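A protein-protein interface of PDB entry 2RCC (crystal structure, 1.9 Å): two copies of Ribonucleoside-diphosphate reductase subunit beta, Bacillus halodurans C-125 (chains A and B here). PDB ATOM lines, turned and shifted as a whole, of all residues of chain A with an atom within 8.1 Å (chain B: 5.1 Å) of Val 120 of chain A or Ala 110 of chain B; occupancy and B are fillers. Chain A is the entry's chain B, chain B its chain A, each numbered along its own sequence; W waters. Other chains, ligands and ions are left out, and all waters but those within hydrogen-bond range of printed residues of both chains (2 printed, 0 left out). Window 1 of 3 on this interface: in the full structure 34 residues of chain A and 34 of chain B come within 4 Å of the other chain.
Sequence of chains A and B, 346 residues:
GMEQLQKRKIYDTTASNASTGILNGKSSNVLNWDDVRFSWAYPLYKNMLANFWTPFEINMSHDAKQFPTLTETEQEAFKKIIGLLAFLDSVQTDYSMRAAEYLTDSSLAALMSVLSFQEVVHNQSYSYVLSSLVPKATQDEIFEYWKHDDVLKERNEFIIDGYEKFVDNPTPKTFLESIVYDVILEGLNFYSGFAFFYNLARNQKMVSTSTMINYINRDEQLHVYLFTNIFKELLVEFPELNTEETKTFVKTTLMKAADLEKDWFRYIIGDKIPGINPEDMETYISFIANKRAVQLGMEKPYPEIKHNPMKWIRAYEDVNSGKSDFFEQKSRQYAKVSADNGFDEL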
ATOM      1  N   PRO A  55      -4.037  -2.293 -12.539  1.00  0.00           N
ATOM      2  CA  PRO A  55      -4.549  -3.115 -13.624  1.00  0.00           C
ATOM      3  C   PRO A  55      -5.770  -3.944 -13.257  1.00  0.00           C
ATOM      4  O   PRO A  55      -6.571  -4.283 -14.119  1.00  0.00           O
ATOM      5  CB  PRO A  55      -3.384  -4.042 -13.939  1.00  0.00           C
ATOM      6  CG  PRO A  55      -2.613  -4.097 -12.725  1.00  0.00           C
ATOM      7  CD  PRO A  55      -2.688  -2.741 -12.142  1.00  0.00           C
ATOM      8  N   ASP A  89      10.651  -3.388 -18.271  1.00  0.00           N
ATOM      9  CA  ASP A  89      10.189  -2.869 -16.939  1.00  0.00           C
ATOM     10  C   ASP A  89      10.690  -3.657 -15.716  1.00  0.00           C
ATOM     11  O   ASP A  89      10.800  -3.070 -14.655  1.00  0.00           O
ATOM     12  CB  ASP A  89       8.690  -2.663 -16.856  1.00  0.00           C
ATOM     13  CG  ASP A  89       8.246  -1.323 -17.408  1.00  0.00           C
ATOM     14  OD1 ASP A  89       9.061  -0.346 -17.486  1.00  0.00           O
ATOM     15  OD2 ASP A  89       7.077  -1.287 -17.833  1.00  0.00           O
ATOM     16  N   SER A  90      10.960  -4.948 -15.844  1.00  0.00           N
ATOM     17  CA  SER A  90      11.582  -5.674 -14.710  1.00  0.00           C
ATOM     18  C   SER A  90      12.976  -5.076 -14.451  1.00  0.00           C
ATOM     19  O   SER A  90      13.382  -4.787 -13.320  1.00  0.00           O
ATOM     20  CB  SER A  90      11.719  -7.175 -14.985  1.00  0.00           C
ATOM     21  OG  SER A  90      10.484  -7.848 -15.003  1.00  0.00           O
ATOM     22  N   GLN A  92      14.113  -2.145 -15.428  1.00  0.00           N
ATOM     23  CA  GLN A  92      13.929  -0.732 -15.043  1.00  0.00           C
ATOM     24  C   GLN A  92      13.508  -0.549 -13.585  1.00  0.00           C
ATOM     25  O   GLN A  92      13.887   0.435 -12.923  1.00  0.00           O
ATOM     26  CB  GLN A  92      12.904  -0.091 -15.997  1.00  0.00           C
ATOM     27  CG  GLN A  92      12.646   1.397 -15.808  1.00  0.00           C
ATOM     28  CD  GLN A  92      13.831   2.262 -16.100  1.00  0.00           C
ATOM     29  OE1 GLN A  92      14.851   1.803 -16.598  1.00  0.00           O
ATOM     30  NE2 GLN A  92      13.709   3.545 -15.788  1.00  0.00           N
ATOM     31  N   THR A  93      12.730  -1.480 -13.067  1.00  0.00           N
ATOM     32  CA  THR A  93      12.382  -1.446 -11.663  1.00  0.00           C
ATOM     33  C   THR A  93      13.646  -1.457 -10.820  1.00  0.00           C
ATOM     34  O   THR A  93      13.774  -0.692  -9.877  1.00  0.00           O
ATOM     35  CB  THR A  93      11.554  -2.661 -11.235  1.00  0.00           C
ATOM     36  OG1 THR A  93      10.291  -2.641 -11.920  1.00  0.00           O
ATOM     37  CG2 THR A  93      11.352  -2.662  -9.695  1.00  0.00           C
ATOM     38  N   ASP A  94      14.578  -2.318 -11.191  1.00  0.00           N
ATOM     39  CA  ASP A  94      15.823  -2.509 -10.460  1.00  0.00           C
ATOM     40  C   ASP A  94      16.782  -1.321 -10.669  1.00  0.00           C
ATOM     41  O   ASP A  94      17.322  -0.790  -9.711  1.00  0.00           O
ATOM     42  CB  ASP A  94      16.466  -3.831 -10.917  1.00  0.00           C
ATOM     43  CG  ASP A  94      17.420  -4.399  -9.919  1.00  0.00           C
ATOM     44  OD1 ASP A  94      17.737  -3.686  -8.943  1.00  0.00           O
ATOM     45  OD2 ASP A  94      17.883  -5.550 -10.133  1.00  0.00           O
ATOM     46  N   SER A  96      16.120   1.779 -11.532  1.00  0.00           N
ATOM     47  CA  SER A  96      15.585   2.952 -10.836  1.00  0.00           C
ATOM     48  C   SER A  96      15.719   2.908  -9.318  1.00  0.00           C
ATOM     49  O   SER A  96      16.021   3.919  -8.686  1.00  0.00           O
ATOM     50  CB  SER A  96      14.142   3.205 -11.266  1.00  0.00           C
ATOM     51  OG  SER A  96      13.309   2.123 -10.932  1.00  0.00           O
ATOM     52  N   MET A  97      15.536   1.736  -8.726  1.00  0.00           N
ATOM     53  CA  MET A  97      15.740   1.559  -7.287  1.00  0.00           C
ATOM     54  C   MET A  97      17.199   1.825  -6.908  1.00  0.00           C
ATOM     55  O   MET A  97      17.475   2.488  -5.923  1.00  0.00           O
ATOM     56  CB  MET A  97      15.258   0.160  -6.852  1.00  0.00           C
ATOM     57  CG  MET A  97      15.441  -0.257  -5.441  1.00  0.00           C
ATOM     58  SD  MET A  97      14.425  -1.882  -5.094  1.00  0.00           S
ATOM     59  CE  MET A  97      14.568  -2.859  -6.712  1.00  0.00           C
ATOM     60  N   SER A 113      12.042   7.096  -6.341  1.00  0.00           N
ATOM     61  CA  SER A 113      11.299   6.037  -5.630  1.00  0.00           C
ATOM     62  C   SER A 113       9.896   5.863  -6.132  1.00  0.00           C
ATOM     63  O   SER A 113       9.429   4.739  -6.251  1.00  0.00           O
ATOM     64  CB  SER A 113      11.256   6.281  -4.130  1.00  0.00           C
ATOM     65  OG  SER A 113      12.575   6.332  -3.641  1.00  0.00           O
ATOM     66  N   VAL A 114       9.210   6.967  -6.399  1.00  0.00           N
ATOM     67  CA  VAL A 114       7.860   6.886  -6.984  1.00  0.00           C
ATOM     68  C   VAL A 114       7.930   6.231  -8.331  1.00  0.00           C
ATOM     69  O   VAL A 114       7.118   5.360  -8.636  1.00  0.00           O
ATOM     70  CB  VAL A 114       7.192   8.280  -7.092  1.00  0.00           C
ATOM     71  CG1 VAL A 114       5.768   8.166  -7.752  1.00  0.00           C
ATOM     72  CG2 VAL A 114       7.109   8.951  -5.704  1.00  0.00           C
ATOM     73  N   LEU A 115       8.941   6.591  -9.130  1.00  0.00           N
ATOM     74  CA  LEU A 115       9.116   6.045 -10.481  1.00  0.00           C
ATOM     75  C   LEU A 115       9.359   4.535 -10.400  1.00  0.00           C
ATOM     76  O   LEU A 115       8.723   3.813 -11.129  1.00  0.00           O
ATOM     77  CB  LEU A 115      10.273   6.749 -11.243  1.00  0.00           C
ATOM     78  CG  LEU A 115      10.634   6.291 -12.679  1.00  0.00           C
ATOM     79  CD1 LEU A 115      11.249   7.468 -13.463  1.00  0.00           C
ATOM     80  CD2 LEU A 115      11.553   5.035 -12.745  1.00  0.00           C
ATOM     81  N   SER A 116      10.233   4.070  -9.498  1.00  0.00           N
ATOM     82  CA  SER A 116      10.500   2.622  -9.329  1.00  0.00           C
ATOM     83  C   SER A 116       9.238   1.844  -8.962  1.00  0.00           C
ATOM     84  O   SER A 116       8.980   0.771  -9.523  1.00  0.00           O
ATOM     85  CB  SER A 116      11.601   2.373  -8.304  1.00  0.00           C
ATOM     86  OG  SER A 116      11.995   0.995  -8.266  1.00  0.00           O
ATOM     87  N   PHE A 117       8.448   2.410  -8.043  1.00  0.00           N
ATOM     88  CA  PHE A 117       7.163   1.835  -7.668  1.00  0.00           C
ATOM     89  C   PHE A 117       6.222   1.732  -8.888  1.00  0.00           C
ATOM     90  O   PHE A 117       5.515   0.705  -9.081  1.00  0.00           O
ATOM     91  CB  PHE A 117       6.461   2.611  -6.558  1.00  0.00           C
ATOM     92  CG  PHE A 117       4.953   2.358  -6.504  1.00  0.00           C
ATOM     93  CD1 PHE A 117       4.460   1.152  -6.005  1.00  0.00           C
ATOM     94  CD2 PHE A 117       4.053   3.327  -6.944  1.00  0.00           C
ATOM     95  CE1 PHE A 117       3.080   0.912  -5.937  1.00  0.00           C
ATOM     96  CE2 PHE A 117       2.684   3.103  -6.900  1.00  0.00           C
ATOM     97  CZ  PHE A 117       2.194   1.888  -6.395  1.00  0.00           C
ATOM     98  N   GLN A 118       6.176   2.776  -9.709  1.00  0.00           N
ATOM     99  CA  GLN A 118       5.308   2.730 -10.930  1.00  0.00           C
ATOM    100  C   GLN A 118       5.720   1.613 -11.908  1.00  0.00           C
ATOM    101  O   GLN A 118       4.854   0.936 -12.513  1.00  0.00           O
ATOM    102  CB  GLN A 118       5.257   4.090 -11.613  1.00  0.00           C
ATOM    103  CG  GLN A 118       4.594   5.135 -10.769  1.00  0.00           C
ATOM    104  CD  GLN A 118       4.422   6.453 -11.453  1.00  0.00           C
ATOM    105  OE1 GLN A 118       5.125   6.785 -12.391  1.00  0.00           O
ATOM    106  NE2 GLN A 118       3.494   7.238 -10.956  1.00  0.00           N
ATOM    107  N   GLU A 119       7.026   1.369 -11.983  1.00  0.00           N
ATOM    108  CA  GLU A 119       7.601   0.298 -12.777  1.00  0.00           C
ATOM    109  C   GLU A 119       7.233  -1.080 -12.240  1.00  0.00           C
ATOM    110  O   GLU A 119       6.956  -1.977 -13.022  1.00  0.00           O
ATOM    111  CB  GLU A 119       9.122   0.415 -12.881  1.00  0.00           C
ATOM    112  CG  GLU A 119       9.726   1.698 -13.483  1.00  0.00           C
ATOM    113  CD  GLU A 119       9.243   2.039 -14.872  1.00  0.00           C
ATOM    114  OE1 GLU A 119       8.297   1.448 -15.392  1.00  0.00           O
ATOM    115  OE2 GLU A 119       9.794   2.971 -15.440  1.00  0.00           O
ATOM    116  N   VAL A 120       7.179  -1.229 -10.915  1.00  0.00           N
ATOM    117  CA  VAL A 120       6.679  -2.463 -10.311  1.00  0.00           C
ATOM    118  C   VAL A 120       5.230  -2.753 -10.827  1.00  0.00           C
ATOM    119  O   VAL A 120       4.947  -3.874 -11.271  1.00  0.00           O
ATOM    120  CB  VAL A 120       6.700  -2.444  -8.750  1.00  0.00           C
ATOM    121  CG1 VAL A 120       5.958  -3.683  -8.199  1.00  0.00           C
ATOM    122  CG2 VAL A 120       8.121  -2.369  -8.197  1.00  0.00           C
ATOM    123  N   VAL A 121       4.362  -1.740 -10.827  1.00  0.00           N
ATOM    124  CA  VAL A 121       2.985  -1.901 -11.266  1.00  0.00           C
ATOM    125  C   VAL A 121       2.885  -2.173 -12.783  1.00  0.00           C
ATOM    126  O   VAL A 121       2.073  -3.035 -13.215  1.00  0.00           O
ATOM    127  CB  VAL A 121       2.064  -0.669 -10.888  1.00  0.00           C
ATOM    128  CG1 VAL A 121       0.615  -0.886 -11.372  1.00  0.00           C
ATOM    129  CG2 VAL A 121       2.109  -0.366  -9.389  1.00  0.00           C
ATOM    130  N   HIS A 122       3.670  -1.442 -13.574  1.00  0.00           N
ATOM    131  CA  HIS A 122       3.715  -1.632 -15.037  1.00  0.00           C
ATOM    132  C   HIS A 122       4.110  -3.048 -15.336  1.00  0.00           C
ATOM    133  O   HIS A 122       3.459  -3.692 -16.108  1.00  0.00           O
ATOM    134  CB  HIS A 122       4.737  -0.736 -15.677  1.00  0.00           C
ATOM    135  CG  HIS A 122       4.396   0.726 -15.628  1.00  0.00           C
ATOM    136  ND1 HIS A 122       5.149   1.681 -16.280  1.00  0.00           N
ATOM    137  CD2 HIS A 122       3.401   1.394 -15.000  1.00  0.00           C
ATOM    138  CE1 HIS A 122       4.643   2.879 -16.035  1.00  0.00           C
ATOM    139  NE2 HIS A 122       3.580   2.733 -15.268  1.00  0.00           N
ATOM    140  N   ASN A 123       5.191  -3.531 -14.707  1.00  0.00           N
ATOM    141  CA  ASN A 123       5.661  -4.886 -14.957  1.00  0.00           C
ATOM    142  C   ASN A 123       4.603  -5.903 -14.567  1.00  0.00           C
ATOM    143  O   ASN A 123       4.314  -6.837 -15.322  1.00  0.00           O
ATOM    144  CB  ASN A 123       6.988  -5.174 -14.251  1.00  0.00           C
ATOM    145  CG  ASN A 123       7.470  -6.567 -14.517  1.00  0.00           C
ATOM    146  OD1 ASN A 123       7.826  -6.897 -15.644  1.00  0.00           O
ATOM    147  ND2 ASN A 123       7.491  -7.392 -13.493  1.00  0.00           N
ATOM    148  N   GLN A 124       3.980  -5.703 -13.402  1.00  0.00           N
ATOM    149  CA  GLN A 124       2.922  -6.590 -12.944  1.00  0.00           C
ATOM    150  C   GLN A 124       1.708  -6.603 -13.875  1.00  0.00           C
ATOM    151  O   GLN A 124       1.053  -7.645 -14.053  1.00  0.00           O
ATOM    152  CB  GLN A 124       2.511  -6.261 -11.502  1.00  0.00           C
ATOM    153  CG  GLN A 124       1.406  -7.150 -10.936  1.00  0.00           C
ATOM    154  CD  GLN A 124      -0.022  -6.612 -11.078  1.00  0.00           C
ATOM    155  OE1 GLN A 124      -0.267  -5.437 -10.888  1.00  0.00           O
ATOM    156  NE2 GLN A 124      -0.966  -7.503 -11.324  1.00  0.00           N
ATOM    157  N   SER A 125       1.400  -5.462 -14.430  1.00  0.00           N
ATOM    158  CA  SER A 125       0.294  -5.352 -15.370  1.00  0.00           C
ATOM    159  C   SER A 125       0.475  -6.271 -16.592  1.00  0.00           C
ATOM    160  O   SER A 125      -0.526  -6.737 -17.171  1.00  0.00           O
ATOM    161  CB  SER A 125       0.114  -3.904 -15.818  1.00  0.00           C
ATOM    162  OG  SER A 125      -0.239  -3.087 -14.723  1.00  0.00           O
ATOM    163  N   TYR A 126       1.728  -6.564 -16.985  1.00  0.00           N
ATOM    164  CA  TYR A 126       1.973  -7.501 -18.131  1.00  0.00           C
ATOM    165  C   TYR A 126       1.669  -8.943 -17.744  1.00  0.00           C
ATOM    166  O   TYR A 126       1.169  -9.692 -18.580  1.00  0.00           O
ATOM    167  CB  TYR A 126       3.388  -7.377 -18.751  1.00  0.00           C
ATOM    168  CG  TYR A 126       3.763  -5.981 -19.049  1.00  0.00           C
ATOM    169  CD1 TYR A 126       2.957  -5.165 -19.833  1.00  0.00           C
ATOM    170  CD2 TYR A 126       4.927  -5.456 -18.550  1.00  0.00           C
ATOM    171  CE1 TYR A 126       3.308  -3.870 -20.073  1.00  0.00           C
ATOM    172  CE2 TYR A 126       5.279  -4.182 -18.792  1.00  0.00           C
ATOM    173  CZ  TYR A 126       4.473  -3.392 -19.536  1.00  0.00           C
ATOM    174  OH  TYR A 126       4.850  -2.113 -19.714  1.00  0.00           O
ATOM    175  N   HIS A 223       8.208   9.970 -16.416  1.00  0.00           N
ATOM    176  CA  HIS A 223       9.507   9.300 -16.207  1.00  0.00           C
ATOM    177  C   HIS A 223      10.643   9.925 -17.087  1.00  0.00           C
ATOM    178  O   HIS A 223      11.763  10.196 -16.604  1.00  0.00           O
ATOM    179  CB  HIS A 223       9.406   7.813 -16.527  1.00  0.00           C
ATOM    180  CG  HIS A 223       8.494   7.040 -15.617  1.00  0.00           C
ATOM    181  ND1 HIS A 223       8.373   5.668 -15.683  1.00  0.00           N
ATOM    182  CD2 HIS A 223       7.697   7.441 -14.596  1.00  0.00           C
ATOM    183  CE1 HIS A 223       7.539   5.261 -14.740  1.00  0.00           C
ATOM    184  NE2 HIS A 223       7.099   6.318 -14.079  1.00  0.00           N
ATOM    185  N   LEU B  31      10.746 -10.623 -13.865  1.00  0.00           N
ATOM    186  CA  LEU B  31       9.692 -10.930 -12.925  1.00  0.00           C
ATOM    187  C   LEU B  31       8.331 -11.240 -13.575  1.00  0.00           C
ATOM    188  O   LEU B  31       7.678 -10.370 -14.117  1.00  0.00           O
ATOM    189  CB  LEU B  31       9.524  -9.808 -11.912  1.00  0.00           C
ATOM    190  CG  LEU B  31       8.433  -9.848 -10.819  1.00  0.00           C
ATOM    191  CD1 LEU B  31       8.337 -11.147 -10.011  1.00  0.00           C
ATOM    192  CD2 LEU B  31       8.635  -8.626  -9.914  1.00  0.00           C
ATOM    193  N   TRP B  33       5.008 -12.463 -12.224  1.00  0.00           N
ATOM    194  CA  TRP B  33       4.316 -12.569 -10.935  1.00  0.00           C
ATOM    195  C   TRP B  33       3.557 -13.903 -10.725  1.00  0.00           C
ATOM    196  O   TRP B  33       3.291 -14.260  -9.581  1.00  0.00           O
ATOM    197  CB  TRP B  33       3.406 -11.354 -10.662  1.00  0.00           C
ATOM    198  CG  TRP B  33       4.150 -10.182 -10.088  1.00  0.00           C
ATOM    199  CD1 TRP B  33       4.574  -9.068 -10.758  1.00  0.00           C
ATOM    200  CD2 TRP B  33       4.560 -10.012  -8.733  1.00  0.00           C
ATOM    201  NE1 TRP B  33       5.210  -8.240  -9.914  1.00  0.00           N
ATOM    202  CE2 TRP B  33       5.214  -8.770  -8.657  1.00  0.00           C
ATOM    203  CE3 TRP B  33       4.442 -10.800  -7.564  1.00  0.00           C
ATOM    204  CZ2 TRP B  33       5.770  -8.282  -7.466  1.00  0.00           C
ATOM    205  CZ3 TRP B  33       4.992 -10.314  -6.366  1.00  0.00           C
ATOM    206  CH2 TRP B  33       5.631  -9.069  -6.326  1.00  0.00           C
ATOM    207  N   TYR B  45       1.806  -8.372  -2.488  1.00  0.00           N
ATOM    208  CA  TYR B  45       1.780  -7.277  -3.428  1.00  0.00           C
ATOM    209  C   TYR B  45       0.369  -6.741  -3.654  1.00  0.00           C
ATOM    210  O   TYR B  45       0.127  -5.527  -3.564  1.00  0.00           O
ATOM    211  CB  TYR B  45       2.412  -7.682  -4.781  1.00  0.00           C
ATOM    212  CG  TYR B  45       2.135  -6.709  -5.894  1.00  0.00           C
ATOM    213  CD1 TYR B  45       2.891  -5.543  -6.069  1.00  0.00           C
ATOM    214  CD2 TYR B  45       1.082  -6.911  -6.754  1.00  0.00           C
ATOM    215  CE1 TYR B  45       2.604  -4.661  -7.084  1.00  0.00           C
ATOM    216  CE2 TYR B  45       0.790  -6.027  -7.713  1.00  0.00           C
ATOM    217  CZ  TYR B  45       1.551  -4.912  -7.901  1.00  0.00           C
ATOM    218  OH  TYR B  45       1.181  -4.073  -8.938  1.00  0.00           O
ATOM    219  N   ASP B 105      16.062 -12.446  -5.354  1.00  0.00           N
ATOM    220  CA  ASP B 105      14.681 -12.808  -5.714  1.00  0.00           C
ATOM    221  C   ASP B 105      14.089 -11.537  -6.240  1.00  0.00           C
ATOM    222  O   ASP B 105      14.014 -10.528  -5.491  1.00  0.00           O
ATOM    223  CB  ASP B 105      13.890 -13.344  -4.518  1.00  0.00           C
ATOM    224  CG  ASP B 105      12.439 -13.754  -4.862  1.00  0.00           C
ATOM    225  OD1 ASP B 105      11.695 -12.946  -5.434  1.00  0.00           O
ATOM    226  OD2 ASP B 105      12.009 -14.852  -4.450  1.00  0.00           O
ATOM    227  N   SER B 106      13.639 -11.578  -7.496  1.00  0.00           N
ATOM    228  CA  SER B 106      13.106 -10.395  -8.163  1.00  0.00           C
ATOM    229  C   SER B 106      11.795  -9.934  -7.563  1.00  0.00           C
ATOM    230  O   SER B 106      11.520  -8.717  -7.574  1.00  0.00           O
ATOM    231  CB  SER B 106      12.947 -10.612  -9.667  1.00  0.00           C
ATOM    232  OG  SER B 106      12.127 -11.717  -9.943  1.00  0.00           O
ATOM    233  N   SER B 107      10.971 -10.878  -7.073  1.00  0.00           N
ATOM    234  CA  SER B 107       9.707 -10.538  -6.416  1.00  0.00           C
ATOM    235  C   SER B 107       9.949  -9.798  -5.104  1.00  0.00           C
ATOM    236  O   SER B 107       9.256  -8.834  -4.806  1.00  0.00           O
ATOM    237  CB  SER B 107       8.763 -11.740  -6.203  1.00  0.00           C
ATOM    238  OG  SER B 107       9.260 -12.635  -5.230  1.00  0.00           O
ATOM    239  N   LEU B 108      10.924 -10.236  -4.312  1.00  0.00           N
ATOM    240  CA  LEU B 108      11.239  -9.551  -3.065  1.00  0.00           C
ATOM    241  C   LEU B 108      11.870  -8.179  -3.343  1.00  0.00           C
ATOM    242  O   LEU B 108      11.565  -7.207  -2.643  1.00  0.00           O
ATOM    243  CB  LEU B 108      12.168 -10.406  -2.179  1.00  0.00           C
ATOM    244  CG  LEU B 108      11.612 -11.792  -1.757  1.00  0.00           C
ATOM    245  CD1 LEU B 108      12.562 -12.512  -0.790  1.00  0.00           C
ATOM    246  CD2 LEU B 108      10.223 -11.699  -1.133  1.00  0.00           C
ATOM    247  N   ALA B 109      12.745  -8.091  -4.356  1.00  0.00           N
ATOM    248  CA  ALA B 109      13.323  -6.796  -4.766  1.00  0.00           C
ATOM    249  C   ALA B 109      12.203  -5.845  -5.149  1.00  0.00           C
ATOM    250  O   ALA B 109      12.219  -4.686  -4.748  1.00  0.00           O
ATOM    251  CB  ALA B 109      14.336  -6.985  -5.889  1.00  0.00           C
ATOM    252  N   ALA B 110      11.203  -6.319  -5.894  1.00  0.00           N
ATOM    253  CA  ALA B 110      10.070  -5.466  -6.274  1.00  0.00           C
ATOM    254  C   ALA B 110       9.285  -4.974  -5.040  1.00  0.00           C
ATOM    255  O   ALA B 110       8.863  -3.791  -4.947  1.00  0.00           O
ATOM    256  CB  ALA B 110       9.142  -6.212  -7.230  1.00  0.00           C
ATOM    257  N   LEU B 111       9.063  -5.867  -4.100  1.00  0.00           N
ATOM    258  CA  LEU B 111       8.334  -5.488  -2.878  1.00  0.00           C
ATOM    259  C   LEU B 111       9.124  -4.446  -2.073  1.00  0.00           C
ATOM    260  O   LEU B 111       8.546  -3.562  -1.473  1.00  0.00           O
ATOM    261  CB  LEU B 111       7.941  -6.729  -2.070  1.00  0.00           C
ATOM    262  CG  LEU B 111       6.874  -7.678  -2.625  1.00  0.00           C
ATOM    263  CD1 LEU B 111       6.907  -9.010  -1.827  1.00  0.00           C
ATOM    264  CD2 LEU B 111       5.497  -6.969  -2.615  1.00  0.00           C
ATOM    265  N   MET B 112      10.440  -4.520  -2.106  1.00  0.00           N
ATOM    266  CA  MET B 112      11.273  -3.486  -1.451  1.00  0.00           C
ATOM    267  C   MET B 112      11.097  -2.132  -2.132  1.00  0.00           C
ATOM    268  O   MET B 112      11.075  -1.114  -1.457  1.00  0.00           O
ATOM    269  CB  MET B 112      12.737  -3.896  -1.375  1.00  0.00           C
ATOM    270  CG  MET B 112      13.051  -5.073  -0.483  1.00  0.00           C
ATOM    271  SD  MET B 112      12.424  -4.908   1.340  1.00  0.00           S
ATOM    272  CE  MET B 112      13.517  -3.395   1.964  1.00  0.00           C
ATOM    273  N   SER B 113      10.903  -2.127  -3.455  1.00  0.00           N
ATOM    274  CA  SER B 113      10.594  -0.902  -4.181  1.00  0.00           C
ATOM    275  C   SER B 113       9.247  -0.314  -3.710  1.00  0.00           C
ATOM    276  O   SER B 113       9.147   0.883  -3.466  1.00  0.00           O
ATOM    277  CB  SER B 113      10.620  -1.135  -5.704  1.00  0.00           C
ATOM    278  OG  SER B 113      10.173  -0.014  -6.407  1.00  0.00           O
ATOM    279  N   VAL B 114       8.228  -1.160  -3.588  1.00  0.00           N
ATOM    280  CA  VAL B 114       6.919  -0.740  -3.105  1.00  0.00           C
ATOM    281  C   VAL B 114       7.081  -0.203  -1.665  1.00  0.00           C
ATOM    282  O   VAL B 114       6.577   0.859  -1.379  1.00  0.00           O
ATOM    283  CB  VAL B 114       5.863  -1.888  -3.156  1.00  0.00           C
ATOM    284  CG1 VAL B 114       4.533  -1.429  -2.527  1.00  0.00           C
ATOM    285  CG2 VAL B 114       5.700  -2.446  -4.572  1.00  0.00           C
HETATM  286  O   HOH W   1       5.275  -9.554 -14.570  1.00  0.00           O
HETATM  287  O   HOH W   2       6.697  -5.960 -10.891  1.00  0.00           O
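Water W1 bridges O of Leu 31 of chain B and O of Asn 123 of chain A.
Water W2 lies within hydrogen-bond range of O of Val 120 of chain A (2.7 Å), NE1 of Trp 33 of chain B (2.9 Å) and ND2 of Asn 123 of chain A (3.1 Å).
Of the 13 printed residues of chain B, 7 touch a printed residue of chain A.
Of the 23 printed residues of chain A, 8 touch a printed residue of chain B.
Among the printed residues, no Asp or Glu carboxylate lies within 4 Å of a Lys or Arg side-chain nitrogen of the other chain.
2 positions are printed for both chains.
Of the 13 pairs that touch across the chains among the printed residues, none has its exchanged pair printed and touching as well.
Among the printed residues, merely in contact across the chains: Met 97 of chain A with Ser 113 of chain B (3.9 Å), Val 120 of chain A with Tyr 45 of chain B (3.7 Å), Val 120 of chain A with Ala 110 of chain B (3.6 Å), Val 120 of chain A with Ser 113 of chain B (3.6 Å), Val 120 of chain A with Val 114 of chain B (3.8 Å), Val 121 of chain A with Tyr 45 of chain B (3.7 Å) and Gln 124 of chain A with Trp 33 of chain B (3.6 Å).
The side-chain amide oxygen (OD1) of Asn 123 of chain A lies within hydrogen-bond range of the side-chain hydroxyl (OG) of Ser 90 of chain A, 2.9 Å away.
The backbone carbonyl oxygen (O) of Thr 93 of chain A is in hydrogen-bond range of the side-chain hydroxyl (OG) of Ser 116 of chain A, at 2.9 Å.
O of Val 121 of chain A lies within hydrogen-bond range of OG of Ser 125 of chain A, 2.8 Å away.
OG of Ser 116 of chain A lies close to OG of Ser 96 of chain A (3.2 Å).
The backbone NH (N) of Leu 31 of chain B is in hydrogen-bond range of the side-chain hydroxyl (OG) of Ser 90 of chain A (3.0 Å).
OG of Ser 116 of chain A is in hydrogen-bond range of OG of Ser 113 of chain B (2.8 Å).
The side-chain hydroxyl (OH) of Tyr 45 of chain B sits at hydrogen-bond distance from the side-chain amide oxygen (OE1) of Gln 124 of chain A (2.8 Å).
The backbone carbonyl oxygen of Ala 109 of chain B lies close to the side-chain sulfur of Met 97 of chain A, at 3.6 Å.
O of Leu 31 of chain B is in hydrogen-bond range of ND2 of Asn 123 of chain A (3.0 Å).
The side-chain hydroxyl (OG) of Ser 113 of chain B lies within hydrogen-bond range of the backbone NH (N) of Phe 117 of chain A, at 3.4 Å.
Of chain B, only Tyr 45, Ala 110, Ser 113 and Val 114 come within 4 Å of Val 120 of chain A.
Printed residues of chain B within 4 Å of Asn 123 of chain A: Leu 31.
Printed residues of chain B within 4 Å of Gln 124 of chain A: Trp 33 (3.6 Å) and Tyr 45 (2.8 Å).
Of chain A, only Met 97 (3.6 Å) comes within 4 Å of Ala 109 of chain B.
Of chain A, only Val 120 comes within 4 Å of Ala 110 of chain B.
Printed residues of chain A within 4 Å of Val 114 of chain B: Val 120.
The nearest residue of chain B that does not touch Val 120 of chain A is Trp 33 of chain B (4.6 Å).
The nearest residue of chain A that does not touch Ala 110 of chain B is Thr 93 of chain A (4.6 Å).
The nearest printed residue of chain B that does not touch Phe 117 of chain A is Val 114 of chain B (4.1 Å).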
